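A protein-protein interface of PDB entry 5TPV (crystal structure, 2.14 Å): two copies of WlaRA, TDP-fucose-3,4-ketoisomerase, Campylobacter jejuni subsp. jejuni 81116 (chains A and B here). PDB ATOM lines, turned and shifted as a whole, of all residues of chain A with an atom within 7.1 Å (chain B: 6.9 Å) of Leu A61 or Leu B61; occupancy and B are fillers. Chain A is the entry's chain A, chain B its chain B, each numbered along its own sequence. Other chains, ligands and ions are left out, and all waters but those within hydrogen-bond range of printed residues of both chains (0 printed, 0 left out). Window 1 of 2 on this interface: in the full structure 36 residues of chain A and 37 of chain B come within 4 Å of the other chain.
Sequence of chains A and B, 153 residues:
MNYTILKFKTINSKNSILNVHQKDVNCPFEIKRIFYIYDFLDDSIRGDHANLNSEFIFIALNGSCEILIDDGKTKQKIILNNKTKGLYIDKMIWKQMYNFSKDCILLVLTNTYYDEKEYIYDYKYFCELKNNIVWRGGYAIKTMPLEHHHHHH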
ATOM      1  N   ASN A  19     -11.682  22.666  31.976  1.00  0.00           N
ATOM      2  CA  ASN A  19     -12.218  21.396  31.457  1.00  0.00           C
ATOM      3  C   ASN A  19     -11.108  20.347  31.309  1.00  0.00           C
ATOM      4  O   ASN A  19     -10.115  20.542  30.561  1.00  0.00           O
ATOM      5  CB  ASN A  19     -12.723  21.567  30.026  1.00  0.00           C
ATOM      6  CG  ASN A  19     -14.078  22.169  29.936  1.00  0.00           C
ATOM      7  OD1 ASN A  19     -14.415  23.032  30.707  1.00  0.00           O
ATOM      8  ND2 ASN A  19     -14.840  21.768  28.957  1.00  0.00           N
ATOM      9  N   HIS A  21      -9.725  16.414  30.479  1.00  0.00           N
ATOM     10  CA  HIS A  21      -9.995  15.130  29.822  1.00  0.00           C
ATOM     11  C   HIS A  21      -8.892  14.075  30.088  1.00  0.00           C
ATOM     12  O   HIS A  21      -7.709  14.323  29.827  1.00  0.00           O
ATOM     13  CB  HIS A  21     -10.203  15.336  28.292  1.00  0.00           C
ATOM     14  CG  HIS A  21     -11.295  16.317  27.973  1.00  0.00           C
ATOM     15  ND1 HIS A  21     -12.604  15.954  27.764  1.00  0.00           N
ATOM     16  CD2 HIS A  21     -11.273  17.667  27.908  1.00  0.00           C
ATOM     17  CE1 HIS A  21     -13.328  17.034  27.539  1.00  0.00           C
ATOM     18  NE2 HIS A  21     -12.540  18.085  27.605  1.00  0.00           N
ATOM     19  N   TYR A  36      -5.590  19.550  16.913  1.00  0.00           N
ATOM     20  CA  TYR A  36      -6.498  20.615  16.662  1.00  0.00           C
ATOM     21  C   TYR A  36      -6.298  21.184  15.236  1.00  0.00           C
ATOM     22  O   TYR A  36      -5.211  21.100  14.682  1.00  0.00           O
ATOM     23  CB  TYR A  36      -6.416  21.698  17.724  1.00  0.00           C
ATOM     24  CG  TYR A  36      -5.043  22.170  18.098  1.00  0.00           C
ATOM     25  CD1 TYR A  36      -4.521  23.344  17.600  1.00  0.00           C
ATOM     26  CD2 TYR A  36      -4.319  21.479  19.043  1.00  0.00           C
ATOM     27  CE1 TYR A  36      -3.264  23.720  17.938  1.00  0.00           C
ATOM     28  CE2 TYR A  36      -3.065  21.872  19.406  1.00  0.00           C
ATOM     29  CZ  TYR A  36      -2.546  22.970  18.845  1.00  0.00           C
ATOM     30  OH  TYR A  36      -1.275  23.314  19.213  1.00  0.00           O
ATOM     31  N   TYR A  38      -7.575  24.404  12.497  1.00  0.00           N
ATOM     32  CA  TYR A  38      -7.932  25.817  12.571  1.00  0.00           C
ATOM     33  C   TYR A  38      -7.611  26.514  11.256  1.00  0.00           C
ATOM     34  O   TYR A  38      -7.127  25.861  10.336  1.00  0.00           O
ATOM     35  CB  TYR A  38      -7.139  26.453  13.731  1.00  0.00           C
ATOM     36  CG  TYR A  38      -5.625  26.264  13.733  1.00  0.00           C
ATOM     37  CD1 TYR A  38      -4.808  27.228  13.177  1.00  0.00           C
ATOM     38  CD2 TYR A  38      -5.005  25.138  14.279  1.00  0.00           C
ATOM     39  CE1 TYR A  38      -3.427  27.092  13.134  1.00  0.00           C
ATOM     40  CE2 TYR A  38      -3.615  24.988  14.235  1.00  0.00           C
ATOM     41  CZ  TYR A  38      -2.828  25.980  13.666  1.00  0.00           C
ATOM     42  OH  TYR A  38      -1.449  25.987  13.605  1.00  0.00           O
ATOM     43  N   ILE A  59     -14.403  18.307  19.651  1.00  0.00           N
ATOM     44  CA  ILE A  59     -14.862  19.389  20.528  1.00  0.00           C
ATOM     45  C   ILE A  59     -14.592  20.699  19.813  1.00  0.00           C
ATOM     46  O   ILE A  59     -13.461  20.916  19.356  1.00  0.00           O
ATOM     47  CB  ILE A  59     -14.182  19.415  21.894  1.00  0.00           C
ATOM     48  CG1 ILE A  59     -14.387  18.114  22.638  1.00  0.00           C
ATOM     49  CG2 ILE A  59     -14.777  20.543  22.726  1.00  0.00           C
ATOM     50  CD1 ILE A  59     -13.244  17.840  23.591  1.00  0.00           C
ATOM     51  N   ALA A  60     -15.620  21.534  19.616  1.00  0.00           N
ATOM     52  CA  ALA A  60     -15.348  22.835  19.081  1.00  0.00           C
ATOM     53  C   ALA A  60     -14.970  23.772  20.211  1.00  0.00           C
ATOM     54  O   ALA A  60     -15.792  24.187  21.022  1.00  0.00           O
ATOM     55  CB  ALA A  60     -16.520  23.358  18.304  1.00  0.00           C
ATOM     56  N   LEU A  61     -13.724  24.202  20.210  1.00  0.00           N
ATOM     57  CA  LEU A  61     -13.251  25.038  21.307  1.00  0.00           C
ATOM     58  C   LEU A  61     -13.494  26.479  21.039  1.00  0.00           C
ATOM     59  O   LEU A  61     -13.662  27.263  21.967  1.00  0.00           O
ATOM     60  CB  LEU A  61     -11.749  24.938  21.523  1.00  0.00           C
ATOM     61  CG  LEU A  61     -11.249  23.695  22.223  1.00  0.00           C
ATOM     62  CD1 LEU A  61      -9.772  23.880  22.479  1.00  0.00           C
ATOM     63  CD2 LEU A  61     -12.014  23.405  23.495  1.00  0.00           C
ATOM     64  N   ASN A  62     -13.478  26.845  19.777  1.00  0.00           N
ATOM     65  CA  ASN A  62     -14.036  28.127  19.388  1.00  0.00           C
ATOM     66  C   ASN A  62     -14.816  27.950  18.101  1.00  0.00           C
ATOM     67  O   ASN A  62     -14.556  27.016  17.327  1.00  0.00           O
ATOM     68  CB  ASN A  62     -12.857  29.057  19.168  1.00  0.00           C
ATOM     69  CG  ASN A  62     -13.222  30.519  19.275  1.00  0.00           C
ATOM     70  OD1 ASN A  62     -13.818  30.942  20.250  1.00  0.00           O
ATOM     71  ND2 ASN A  62     -12.825  31.292  18.282  1.00  0.00           N
ATOM     72  N   GLY A  63     -15.773  28.843  17.874  1.00  0.00           N
ATOM     73  CA  GLY A  63     -16.636  28.749  16.686  1.00  0.00           C
ATOM     74  C   GLY A  63     -17.363  27.417  16.575  1.00  0.00           C
ATOM     75  O   GLY A  63     -17.770  26.837  17.551  1.00  0.00           O
ATOM     76  N   SER A  64     -17.542  26.897  15.388  1.00  0.00           N
ATOM     77  CA  SER A  64     -18.444  25.791  15.299  1.00  0.00           C
ATOM     78  C   SER A  64     -18.228  25.136  13.941  1.00  0.00           C
ATOM     79  O   SER A  64     -17.615  25.723  13.074  1.00  0.00           O
ATOM     80  CB  SER A  64     -19.893  26.337  15.369  1.00  0.00           C
ATOM     81  OG  SER A  64     -20.168  27.096  14.193  1.00  0.00           O
ATOM     82  N   LEU A  80     -21.240  21.038  16.285  1.00  0.00           N
ATOM     83  CA  LEU A  80     -20.341  21.294  17.402  1.00  0.00           C
ATOM     84  C   LEU A  80     -20.042  22.765  17.516  1.00  0.00           C
ATOM     85  O   LEU A  80     -19.487  23.396  16.602  1.00  0.00           O
ATOM     86  CB  LEU A  80     -18.983  20.633  17.146  1.00  0.00           C
ATOM     87  CG  LEU A  80     -19.091  19.141  16.818  1.00  0.00           C
ATOM     88  CD1 LEU A  80     -17.858  18.668  16.064  1.00  0.00           C
ATOM     89  CD2 LEU A  80     -19.304  18.392  18.116  1.00  0.00           C
ATOM     90  N   ASN A  81     -20.377  23.299  18.671  1.00  0.00           N
ATOM     91  CA  ASN A  81     -20.241  24.725  18.889  1.00  0.00           C
ATOM     92  C   ASN A  81     -20.111  25.118  20.361  1.00  0.00           C
ATOM     93  O   ASN A  81     -20.534  26.196  20.748  1.00  0.00           O
ATOM     94  CB  ASN A  81     -21.508  25.387  18.327  1.00  0.00           C
ATOM     95  CG  ASN A  81     -22.797  24.935  19.012  1.00  0.00           C
ATOM     96  OD1 ASN A  81     -22.846  24.030  19.851  1.00  0.00           O
ATOM     97  ND2 ASN A  81     -23.887  25.554  18.591  1.00  0.00           N
ATOM     98  N   ASN A  82     -19.626  24.219  21.216  1.00  0.00           N
ATOM     99  CA  ASN A  82     -19.781  24.409  22.639  1.00  0.00           C
ATOM    100  C   ASN A  82     -18.606  23.735  23.388  1.00  0.00           C
ATOM    101  O   ASN A  82     -18.312  22.575  23.147  1.00  0.00           O
ATOM    102  CB  ASN A  82     -21.073  23.740  22.984  1.00  0.00           C
ATOM    103  CG  ASN A  82     -21.551  24.131  24.339  1.00  0.00           C
ATOM    104  OD1 ASN A  82     -20.834  24.076  25.326  1.00  0.00           O
ATOM    105  ND2 ASN A  82     -22.798  24.485  24.390  1.00  0.00           N
ATOM    106  N   LYS A  83     -17.973  24.464  24.297  1.00  0.00           N
ATOM    107  CA  LYS A  83     -16.847  23.914  25.024  1.00  0.00           C
ATOM    108  C   LYS A  83     -17.212  22.866  26.041  1.00  0.00           C
ATOM    109  O   LYS A  83     -16.299  22.177  26.463  1.00  0.00           O
ATOM    110  CB  LYS A  83     -16.043  24.988  25.735  1.00  0.00           C
ATOM    111  CG  LYS A  83     -15.261  25.883  24.796  1.00  0.00           C
ATOM    112  CD  LYS A  83     -14.966  27.111  25.622  1.00  0.00           C
ATOM    113  CE  LYS A  83     -14.042  28.079  24.942  1.00  0.00           C
ATOM    114  NZ  LYS A  83     -14.736  28.827  23.870  1.00  0.00           N
ATOM    115  N   ASP A 103     -13.673  31.287  12.579  1.00  0.00           N
ATOM    116  CA  ASP A 103     -12.866  31.332  13.774  1.00  0.00           C
ATOM    117  C   ASP A 103     -12.823  29.932  14.442  1.00  0.00           C
ATOM    118  O   ASP A 103     -12.447  29.855  15.626  1.00  0.00           O
ATOM    119  CB  ASP A 103     -13.503  32.389  14.695  1.00  0.00           C
ATOM    120  CG  ASP A 103     -14.970  32.108  15.013  1.00  0.00           C
ATOM    121  OD1 ASP A 103     -15.514  32.605  16.037  1.00  0.00           O
ATOM    122  OD2 ASP A 103     -15.618  31.374  14.236  1.00  0.00           O
ATOM    123  N   CYS A 104     -13.258  28.863  13.741  1.00  0.00           N
ATOM    124  CA  CYS A 104     -13.450  27.578  14.394  1.00  0.00           C
ATOM    125  C   CYS A 104     -12.043  27.072  14.832  1.00  0.00           C
ATOM    126  O   CYS A 104     -11.063  27.213  14.125  1.00  0.00           O
ATOM    127  CB  CYS A 104     -14.138  26.532  13.507  1.00  0.00           C
ATOM    128  SG  CYS A 104     -14.341  24.888  14.285  1.00  0.00           S
ATOM    129  N   ILE A 105     -11.954  26.521  16.031  1.00  0.00           N
ATOM    130  CA  ILE A 105     -10.811  25.681  16.412  1.00  0.00           C
ATOM    131  C   ILE A 105     -11.404  24.365  16.860  1.00  0.00           C
ATOM    132  O   ILE A 105     -12.154  24.349  17.835  1.00  0.00           O
ATOM    133  CB  ILE A 105     -10.039  26.370  17.559  1.00  0.00           C
ATOM    134  CG1 ILE A 105      -9.508  27.732  17.119  1.00  0.00           C
ATOM    135  CG2 ILE A 105      -8.893  25.505  18.040  1.00  0.00           C
ATOM    136  CD1 ILE A 105      -8.923  28.554  18.247  1.00  0.00           C
ATOM    137  N   LEU A 106     -11.074  23.278  16.172  1.00  0.00           N
ATOM    138  CA  LEU A 106     -11.577  21.953  16.477  1.00  0.00           C
ATOM    139  C   LEU A 106     -10.523  21.133  17.190  1.00  0.00           C
ATOM    140  O   LEU A 106      -9.416  21.001  16.668  1.00  0.00           O
ATOM    141  CB  LEU A 106     -11.913  21.234  15.193  1.00  0.00           C
ATOM    142  CG  LEU A 106     -12.390  19.780  15.340  1.00  0.00           C
ATOM    143  CD1 LEU A 106     -13.796  19.665  15.871  1.00  0.00           C
ATOM    144  CD2 LEU A 106     -12.345  19.117  13.981  1.00  0.00           C
ATOM    145  N   LEU A 107     -10.881  20.570  18.347  1.00  0.00           N
ATOM    146  CA  LEU A 107      -9.956  19.807  19.144  1.00  0.00           C
ATOM    147  C   LEU A 107     -10.458  18.407  19.060  1.00  0.00           C
ATOM    148  O   LEU A 107     -11.667  18.167  19.205  1.00  0.00           O
ATOM    149  CB  LEU A 107      -9.849  20.310  20.575  1.00  0.00           C
ATOM    150  CG  LEU A 107      -9.054  19.455  21.592  1.00  0.00           C
ATOM    151  CD1 LEU A 107      -7.563  19.518  21.424  1.00  0.00           C
ATOM    152  CD2 LEU A 107      -9.284  19.817  23.033  1.00  0.00           C
ATOM    153  N   ASN B  19      -2.517  20.718  13.806  1.00  0.00           N
ATOM    154  CA  ASN B  19      -1.379  20.545  14.747  1.00  0.00           C
ATOM    155  C   ASN B  19      -1.547  19.276  15.516  1.00  0.00           C
ATOM    156  O   ASN B  19      -2.507  19.161  16.292  1.00  0.00           O
ATOM    157  CB  ASN B  19      -1.284  21.611  15.849  1.00  0.00           C
ATOM    158  CG  ASN B  19      -0.770  22.941  15.364  1.00  0.00           C
ATOM    159  OD1 ASN B  19      -0.854  23.248  14.182  1.00  0.00           O
ATOM    160  ND2 ASN B  19      -0.349  23.793  16.291  1.00  0.00           N
ATOM    161  N   HIS B  21      -0.264  16.381  18.348  1.00  0.00           N
ATOM    162  CA  HIS B  21       0.566  16.168  19.530  1.00  0.00           C
ATOM    163  C   HIS B  21       0.396  14.759  20.038  1.00  0.00           C
ATOM    164  O   HIS B  21      -0.700  14.282  20.398  1.00  0.00           O
ATOM    165  CB  HIS B  21       0.254  17.148  20.663  1.00  0.00           C
ATOM    166  CG  HIS B  21       0.369  18.571  20.266  1.00  0.00           C
ATOM    167  ND1 HIS B  21       1.541  19.280  20.362  1.00  0.00           N
ATOM    168  CD2 HIS B  21      -0.549  19.432  19.779  1.00  0.00           C
ATOM    169  CE1 HIS B  21       1.359  20.500  19.905  1.00  0.00           C
ATOM    170  NE2 HIS B  21       0.090  20.630  19.573  1.00  0.00           N
ATOM    171  N   TYR B  36      -8.084  22.406  29.332  1.00  0.00           N
ATOM    172  CA  TYR B  36      -8.103  23.748  28.767  1.00  0.00           C
ATOM    173  C   TYR B  36      -8.906  24.634  29.709  1.00  0.00           C
ATOM    174  O   TYR B  36      -9.836  24.189  30.416  1.00  0.00           O
ATOM    175  CB  TYR B  36      -8.569  23.792  27.274  1.00  0.00           C
ATOM    176  CG  TYR B  36      -9.785  22.971  26.999  1.00  0.00           C
ATOM    177  CD1 TYR B  36     -11.055  23.540  27.038  1.00  0.00           C
ATOM    178  CD2 TYR B  36      -9.690  21.618  26.678  1.00  0.00           C
ATOM    179  CE1 TYR B  36     -12.172  22.788  26.837  1.00  0.00           C
ATOM    180  CE2 TYR B  36     -10.824  20.867  26.475  1.00  0.00           C
ATOM    181  CZ  TYR B  36     -12.049  21.453  26.575  1.00  0.00           C
ATOM    182  OH  TYR B  36     -13.186  20.708  26.361  1.00  0.00           O
ATOM    183  N   TYR B  38     -10.455  28.704  30.189  1.00  0.00           N
ATOM    184  CA  TYR B  38     -11.062  29.736  29.351  1.00  0.00           C
ATOM    185  C   TYR B  38     -12.033  30.607  30.169  1.00  0.00           C
ATOM    186  O   TYR B  38     -12.230  30.374  31.371  1.00  0.00           O
ATOM    187  CB  TYR B  38     -11.770  29.038  28.194  1.00  0.00           C
ATOM    188  CG  TYR B  38     -12.822  28.002  28.610  1.00  0.00           C
ATOM    189  CD1 TYR B  38     -14.165  28.325  28.735  1.00  0.00           C
ATOM    190  CD2 TYR B  38     -12.469  26.692  28.802  1.00  0.00           C
ATOM    191  CE1 TYR B  38     -15.107  27.401  29.139  1.00  0.00           C
ATOM    192  CE2 TYR B  38     -13.400  25.739  29.149  1.00  0.00           C
ATOM    193  CZ  TYR B  38     -14.701  26.092  29.339  1.00  0.00           C
ATOM    194  OH  TYR B  38     -15.576  25.052  29.698  1.00  0.00           O
ATOM    195  N   ILE B  59      -0.116  25.973  25.756  1.00  0.00           N
ATOM    196  CA  ILE B  59      -0.356  26.560  24.441  1.00  0.00           C
ATOM    197  C   ILE B  59      -1.526  27.519  24.567  1.00  0.00           C
ATOM    198  O   ILE B  59      -2.589  27.143  25.111  1.00  0.00           O
ATOM    199  CB  ILE B  59      -0.726  25.424  23.464  1.00  0.00           C
ATOM    200  CG1 ILE B  59       0.308  24.322  23.467  1.00  0.00           C
ATOM    201  CG2 ILE B  59      -0.944  25.912  22.040  1.00  0.00           C
ATOM    202  CD1 ILE B  59      -0.166  23.058  22.797  1.00  0.00           C
ATOM    203  N   ALA B  60      -1.325  28.761  24.100  1.00  0.00           N
ATOM    204  CA  ALA B  60      -2.413  29.676  23.917  1.00  0.00           C
ATOM    205  C   ALA B  60      -3.058  29.415  22.565  1.00  0.00           C
ATOM    206  O   ALA B  60      -2.568  29.902  21.559  1.00  0.00           O
ATOM    207  CB  ALA B  60      -1.912  31.104  24.019  1.00  0.00           C
ATOM    208  N   LEU B  61      -4.110  28.616  22.539  1.00  0.00           N
ATOM    209  CA  LEU B  61      -4.846  28.342  21.314  1.00  0.00           C
ATOM    210  C   LEU B  61      -5.574  29.532  20.816  1.00  0.00           C
ATOM    211  O   LEU B  61      -5.794  29.665  19.650  1.00  0.00           O
ATOM    212  CB  LEU B  61      -5.953  27.341  21.531  1.00  0.00           C
ATOM    213  CG  LEU B  61      -5.567  25.917  21.826  1.00  0.00           C
ATOM    214  CD1 LEU B  61      -6.780  25.028  21.710  1.00  0.00           C
ATOM    215  CD2 LEU B  61      -4.495  25.453  20.870  1.00  0.00           C
ATOM    216  N   ASN B  62      -6.024  30.378  21.721  1.00  0.00           N
ATOM    217  CA  ASN B  62      -6.518  31.649  21.289  1.00  0.00           C
ATOM    218  C   ASN B  62      -6.104  32.734  22.273  1.00  0.00           C
ATOM    219  O   ASN B  62      -5.828  32.465  23.428  1.00  0.00           O
ATOM    220  CB  ASN B  62      -8.034  31.543  21.080  1.00  0.00           C
ATOM    221  CG  ASN B  62      -8.550  32.575  20.080  1.00  0.00           C
ATOM    222  OD1 ASN B  62      -7.971  32.804  19.015  1.00  0.00           O
ATOM    223  ND2 ASN B  62      -9.603  33.261  20.474  1.00  0.00           N
ATOM    224  N   GLY B  63      -6.011  33.960  21.810  1.00  0.00           N
ATOM    225  CA  GLY B  63      -5.528  35.046  22.648  1.00  0.00           C
ATOM    226  C   GLY B  63      -4.107  34.887  23.158  1.00  0.00           C
ATOM    227  O   GLY B  63      -3.225  34.292  22.543  1.00  0.00           O
ATOM    228  N   ASN B  81       1.129  33.459  23.006  1.00  0.00           N
ATOM    229  CA  ASN B  81       0.192  34.163  22.145  1.00  0.00           C
ATOM    230  C   ASN B  81      -0.034  33.644  20.734  1.00  0.00           C
ATOM    231  O   ASN B  81      -0.654  34.343  19.940  1.00  0.00           O
ATOM    232  CB  ASN B  81       0.531  35.665  22.050  1.00  0.00           C
ATOM    233  CG  ASN B  81       1.894  35.958  21.437  1.00  0.00           C
ATOM    234  OD1 ASN B  81       2.369  37.082  21.561  1.00  0.00           O
ATOM    235  ND2 ASN B  81       2.545  34.992  20.843  1.00  0.00           N
ATOM    236  N   ASN B  82       0.458  32.478  20.387  1.00  0.00           N
ATOM    237  CA  ASN B  82      -0.055  31.874  19.170  1.00  0.00           C
ATOM    238  C   ASN B  82       0.005  30.369  19.134  1.00  0.00           C
ATOM    239  O   ASN B  82       0.686  29.754  19.942  1.00  0.00           O
ATOM    240  CB  ASN B  82       0.631  32.439  17.935  1.00  0.00           C
ATOM    241  CG  ASN B  82       1.967  31.802  17.704  1.00  0.00           C
ATOM    242  OD1 ASN B  82       2.840  31.970  18.510  1.00  0.00           O
ATOM    243  ND2 ASN B  82       2.136  31.110  16.599  1.00  0.00           N
ATOM    244  N   LYS B  83      -0.711  29.815  18.163  1.00  0.00           N
ATOM    245  CA  LYS B  83      -0.986  28.374  18.071  1.00  0.00           C
ATOM    246  C   LYS B  83       0.171  27.544  17.590  1.00  0.00           C
ATOM    247  O   LYS B  83       0.071  26.327  17.603  1.00  0.00           O
ATOM    248  CB  LYS B  83      -2.133  28.118  17.096  1.00  0.00           C
ATOM    249  CG  LYS B  83      -3.480  28.333  17.722  1.00  0.00           C
ATOM    250  CD  LYS B  83      -4.585  27.988  16.736  1.00  0.00           C
ATOM    251  CE  LYS B  83      -5.138  29.207  16.018  1.00  0.00           C
ATOM    252  NZ  LYS B  83      -5.551  30.237  17.002  1.00  0.00           N
ATOM    253  N   LYS B  85       3.317  27.652  18.789  1.00  0.00           N
ATOM    254  CA  LYS B  85       4.336  27.665  19.820  1.00  0.00           C
ATOM    255  C   LYS B  85       3.687  27.224  21.153  1.00  0.00           C
ATOM    256  O   LYS B  85       2.485  27.448  21.438  1.00  0.00           O
ATOM    257  CB  LYS B  85       4.958  29.055  19.852  1.00  0.00           C
ATOM    258  CG  LYS B  85       4.688  29.928  21.063  1.00  0.00           C
ATOM    259  CD  LYS B  85       5.229  31.342  20.812  1.00  0.00           C
ATOM    260  CE  LYS B  85       4.937  32.304  21.952  1.00  0.00           C
ATOM    261  NZ  LYS B  85       6.103  32.310  22.879  1.00  0.00           N
ATOM    262  N   ASP B 103     -10.501  36.632  25.509  1.00  0.00           N
ATOM    263  CA  ASP B 103     -10.654  35.547  24.555  1.00  0.00           C
ATOM    264  C   ASP B 103      -9.586  34.440  24.680  1.00  0.00           C
ATOM    265  O   ASP B 103      -9.572  33.535  23.853  1.00  0.00           O
ATOM    266  CB  ASP B 103     -10.581  36.108  23.115  1.00  0.00           C
ATOM    267  CG  ASP B 103      -9.321  36.922  22.823  1.00  0.00           C
ATOM    268  OD1 ASP B 103      -9.080  37.280  21.644  1.00  0.00           O
ATOM    269  OD2 ASP B 103      -8.552  37.215  23.748  1.00  0.00           O
ATOM    270  N   CYS B 104      -8.708  34.488  25.677  1.00  0.00           N
ATOM    271  CA  CYS B 104      -7.664  33.491  25.836  1.00  0.00           C
ATOM    272  C   CYS B 104      -8.298  32.104  26.012  1.00  0.00           C
ATOM    273  O   CYS B 104      -9.234  31.919  26.750  1.00  0.00           O
ATOM    274  CB  CYS B 104      -6.746  33.748  27.016  1.00  0.00           C
ATOM    275  SG  CYS B 104      -5.349  32.569  26.991  1.00  0.00           S
ATOM    276  N   ILE B 105      -7.795  31.137  25.274  1.00  0.00           N
ATOM    277  CA  ILE B 105      -8.023  29.723  25.586  1.00  0.00           C
ATOM    278  C   ILE B 105      -6.676  29.072  25.784  1.00  0.00           C
ATOM    279  O   ILE B 105      -5.830  29.067  24.881  1.00  0.00           O
ATOM    280  CB  ILE B 105      -8.738  28.968  24.447  1.00  0.00           C
ATOM    281  CG1 ILE B 105     -10.111  29.623  24.203  1.00  0.00           C
ATOM    282  CG2 ILE B 105      -8.882  27.464  24.737  1.00  0.00           C
ATOM    283  CD1 ILE B 105     -10.661  29.265  22.817  1.00  0.00           C
ATOM    284  N   LEU B 106      -6.488  28.501  26.963  1.00  0.00           N
ATOM    285  CA  LEU B 106      -5.197  27.918  27.319  1.00  0.00           C
ATOM    286  C   LEU B 106      -5.360  26.432  27.282  1.00  0.00           C
ATOM    287  O   LEU B 106      -6.200  25.920  27.997  1.00  0.00           O
ATOM    288  CB  LEU B 106      -4.772  28.313  28.738  1.00  0.00           C
ATOM    289  CG  LEU B 106      -3.443  27.689  29.184  1.00  0.00           C
ATOM    290  CD1 LEU B 106      -2.277  28.268  28.446  1.00  0.00           C
ATOM    291  CD2 LEU B 106      -3.271  27.927  30.685  1.00  0.00           C
ATOM    292  N   LEU B 107      -4.568  25.768  26.442  1.00  0.00           N
ATOM    293  CA  LEU B 107      -4.520  24.319  26.416  1.00  0.00           C
ATOM    294  C   LEU B 107      -3.209  23.815  27.046  1.00  0.00           C
ATOM    295  O   LEU B 107      -2.107  24.272  26.698  1.00  0.00           O
ATOM    296  CB  LEU B 107      -4.604  23.860  24.983  1.00  0.00           C
ATOM    297  CG  LEU B 107      -4.470  22.379  24.644  1.00  0.00           C
ATOM    298  CD1 LEU B 107      -5.602  21.566  25.204  1.00  0.00           C
ATOM    299  CD2 LEU B 107      -4.333  22.125  23.142  1.00  0.00           C
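Asn A19 touches Tyr B38, and with the chains exchanged Tyr A38 touches Asn B19.
Tyr A36 touches Ile B59, and with the chains exchanged Ile A59 touches Tyr B36.
Tyr A36 touches Leu B61, and with the chains exchanged Leu A61 touches Tyr B36.
Tyr A36 touches Lys B83, and with the chains exchanged Lys A83 touches Tyr B36.
Printed residues of chain A that touch a printed residue of chain B: Asn A19, His A21, Tyr A36, Tyr A38, Ile A59, Leu A61, Lys A83, Ile A105 and Leu A107.
Of the 18 printed residues of chain B, 9 touch a printed residue of chain A.
Hydrophobic or aromatic side chains of chain B that line the printed part of chain A: His B21, Tyr B36, Tyr B38, Ile B59, Leu B61, Ile B105 and Leu B107.
Among the printed residues, no Asp or Glu carboxylate lies within 4 Å of a Lys or Arg side-chain nitrogen of the other chain.
O of Lys A83 lies within hydrogen-bond range of ND2 of Asn A19, at 2.9 Å.
The backbone NH (N) of Ile A105 is in hydrogen-bond range of the backbone carbonyl oxygen (O) of Asn A62 (2.9 Å).
N of Ile A59 lies within hydrogen-bond range of O of Leu A107 (2.8 Å).
O of Ile B59 is in hydrogen-bond range of N of Leu B107 (2.8 Å).
The side-chain amino group (NZ) of Lys A83 is in hydrogen-bond range of the backbone carbonyl oxygen (O) of Leu A61.
The backbone carbonyl oxygen of Asn B62 lies within hydrogen-bond range of the backbone NH of Ile B105, 3.0 Å away.
Of the printed residues of chain B, Asn A19 touches Tyr B36 and Tyr B38.
Of chain B, only Tyr B36, Leu B61 and Ile B105 come within 4 Å of Leu A61.
Of the printed residues of chain A, Tyr B36 touches Asn A19, His A21, Ile A59, Leu A61, Lys A83 and Leu A107.
Of the printed residues of chain A, Ile B59 touches Tyr A36 (3.8 Å).
Leu B61 touches just these residues of chain A: Tyr A36 (3.6 Å), Leu A61 (3.3 Å) and Ile A105 (3.6 Å).
Of the printed residues of chain A, Ile B105 touches Leu A61.
Of the printed residues of chain A, Leu B107 touches Tyr A36 (3.95 Å).
The nearest printed residue of chain A that does not touch Asn B19 is Leu A106 (7.2 Å).
Tyr A36 touches Ile B59 (OH to CD1, 3.8 Å).
Tyr A36 touches Leu B61.
Tyr A36 touches Lys B83.
Tyr A38 touches Lys B83 (CD1 to CE, 3.5 Å).
Tyr B36 touches Ile A59.
CD2 of Leu A61 touches CE1 of Tyr B36, at 3.4 Å.
CD1 of Leu B61 touches CD1 of Leu A61, 3.3 Å away.
Lys A83 touches Tyr B38 (CD to CD1, 3.4 Å).
Ile A105 touches Leu B61.
Tyr B36 touches Leu A107 (CE2 to CD2, 3.9 Å).
OH of Tyr A38 lies within hydrogen-bond range of OD1 of Asn B19, 2.9 Å away.
OD1 of Asn A19 sits at hydrogen-bond distance from OH of Tyr B38 (2.5 Å).
The backbone carbonyl oxygen (O) of Lys A83 is in hydrogen-bond range of the side-chain hydroxyl (OH) of Tyr B36, 3.4 Å away.
N of Asn A19 is in hydrogen-bond range of O of Tyr B36, 2.9 Å away.
OH of Tyr B36 is in hydrogen-bond range of NE2 of His A21, 3.0 Å away.
The backbone carbonyl oxygen (O) of Tyr A36 lies within hydrogen-bond range of the backbone NH (N) of Asn B19, at 2.9 Å.
The side-chain hydroxyl (OH) of Tyr A36 sits at hydrogen-bond distance from a ring nitrogen (NE2) of His B21, at 3.0 Å.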
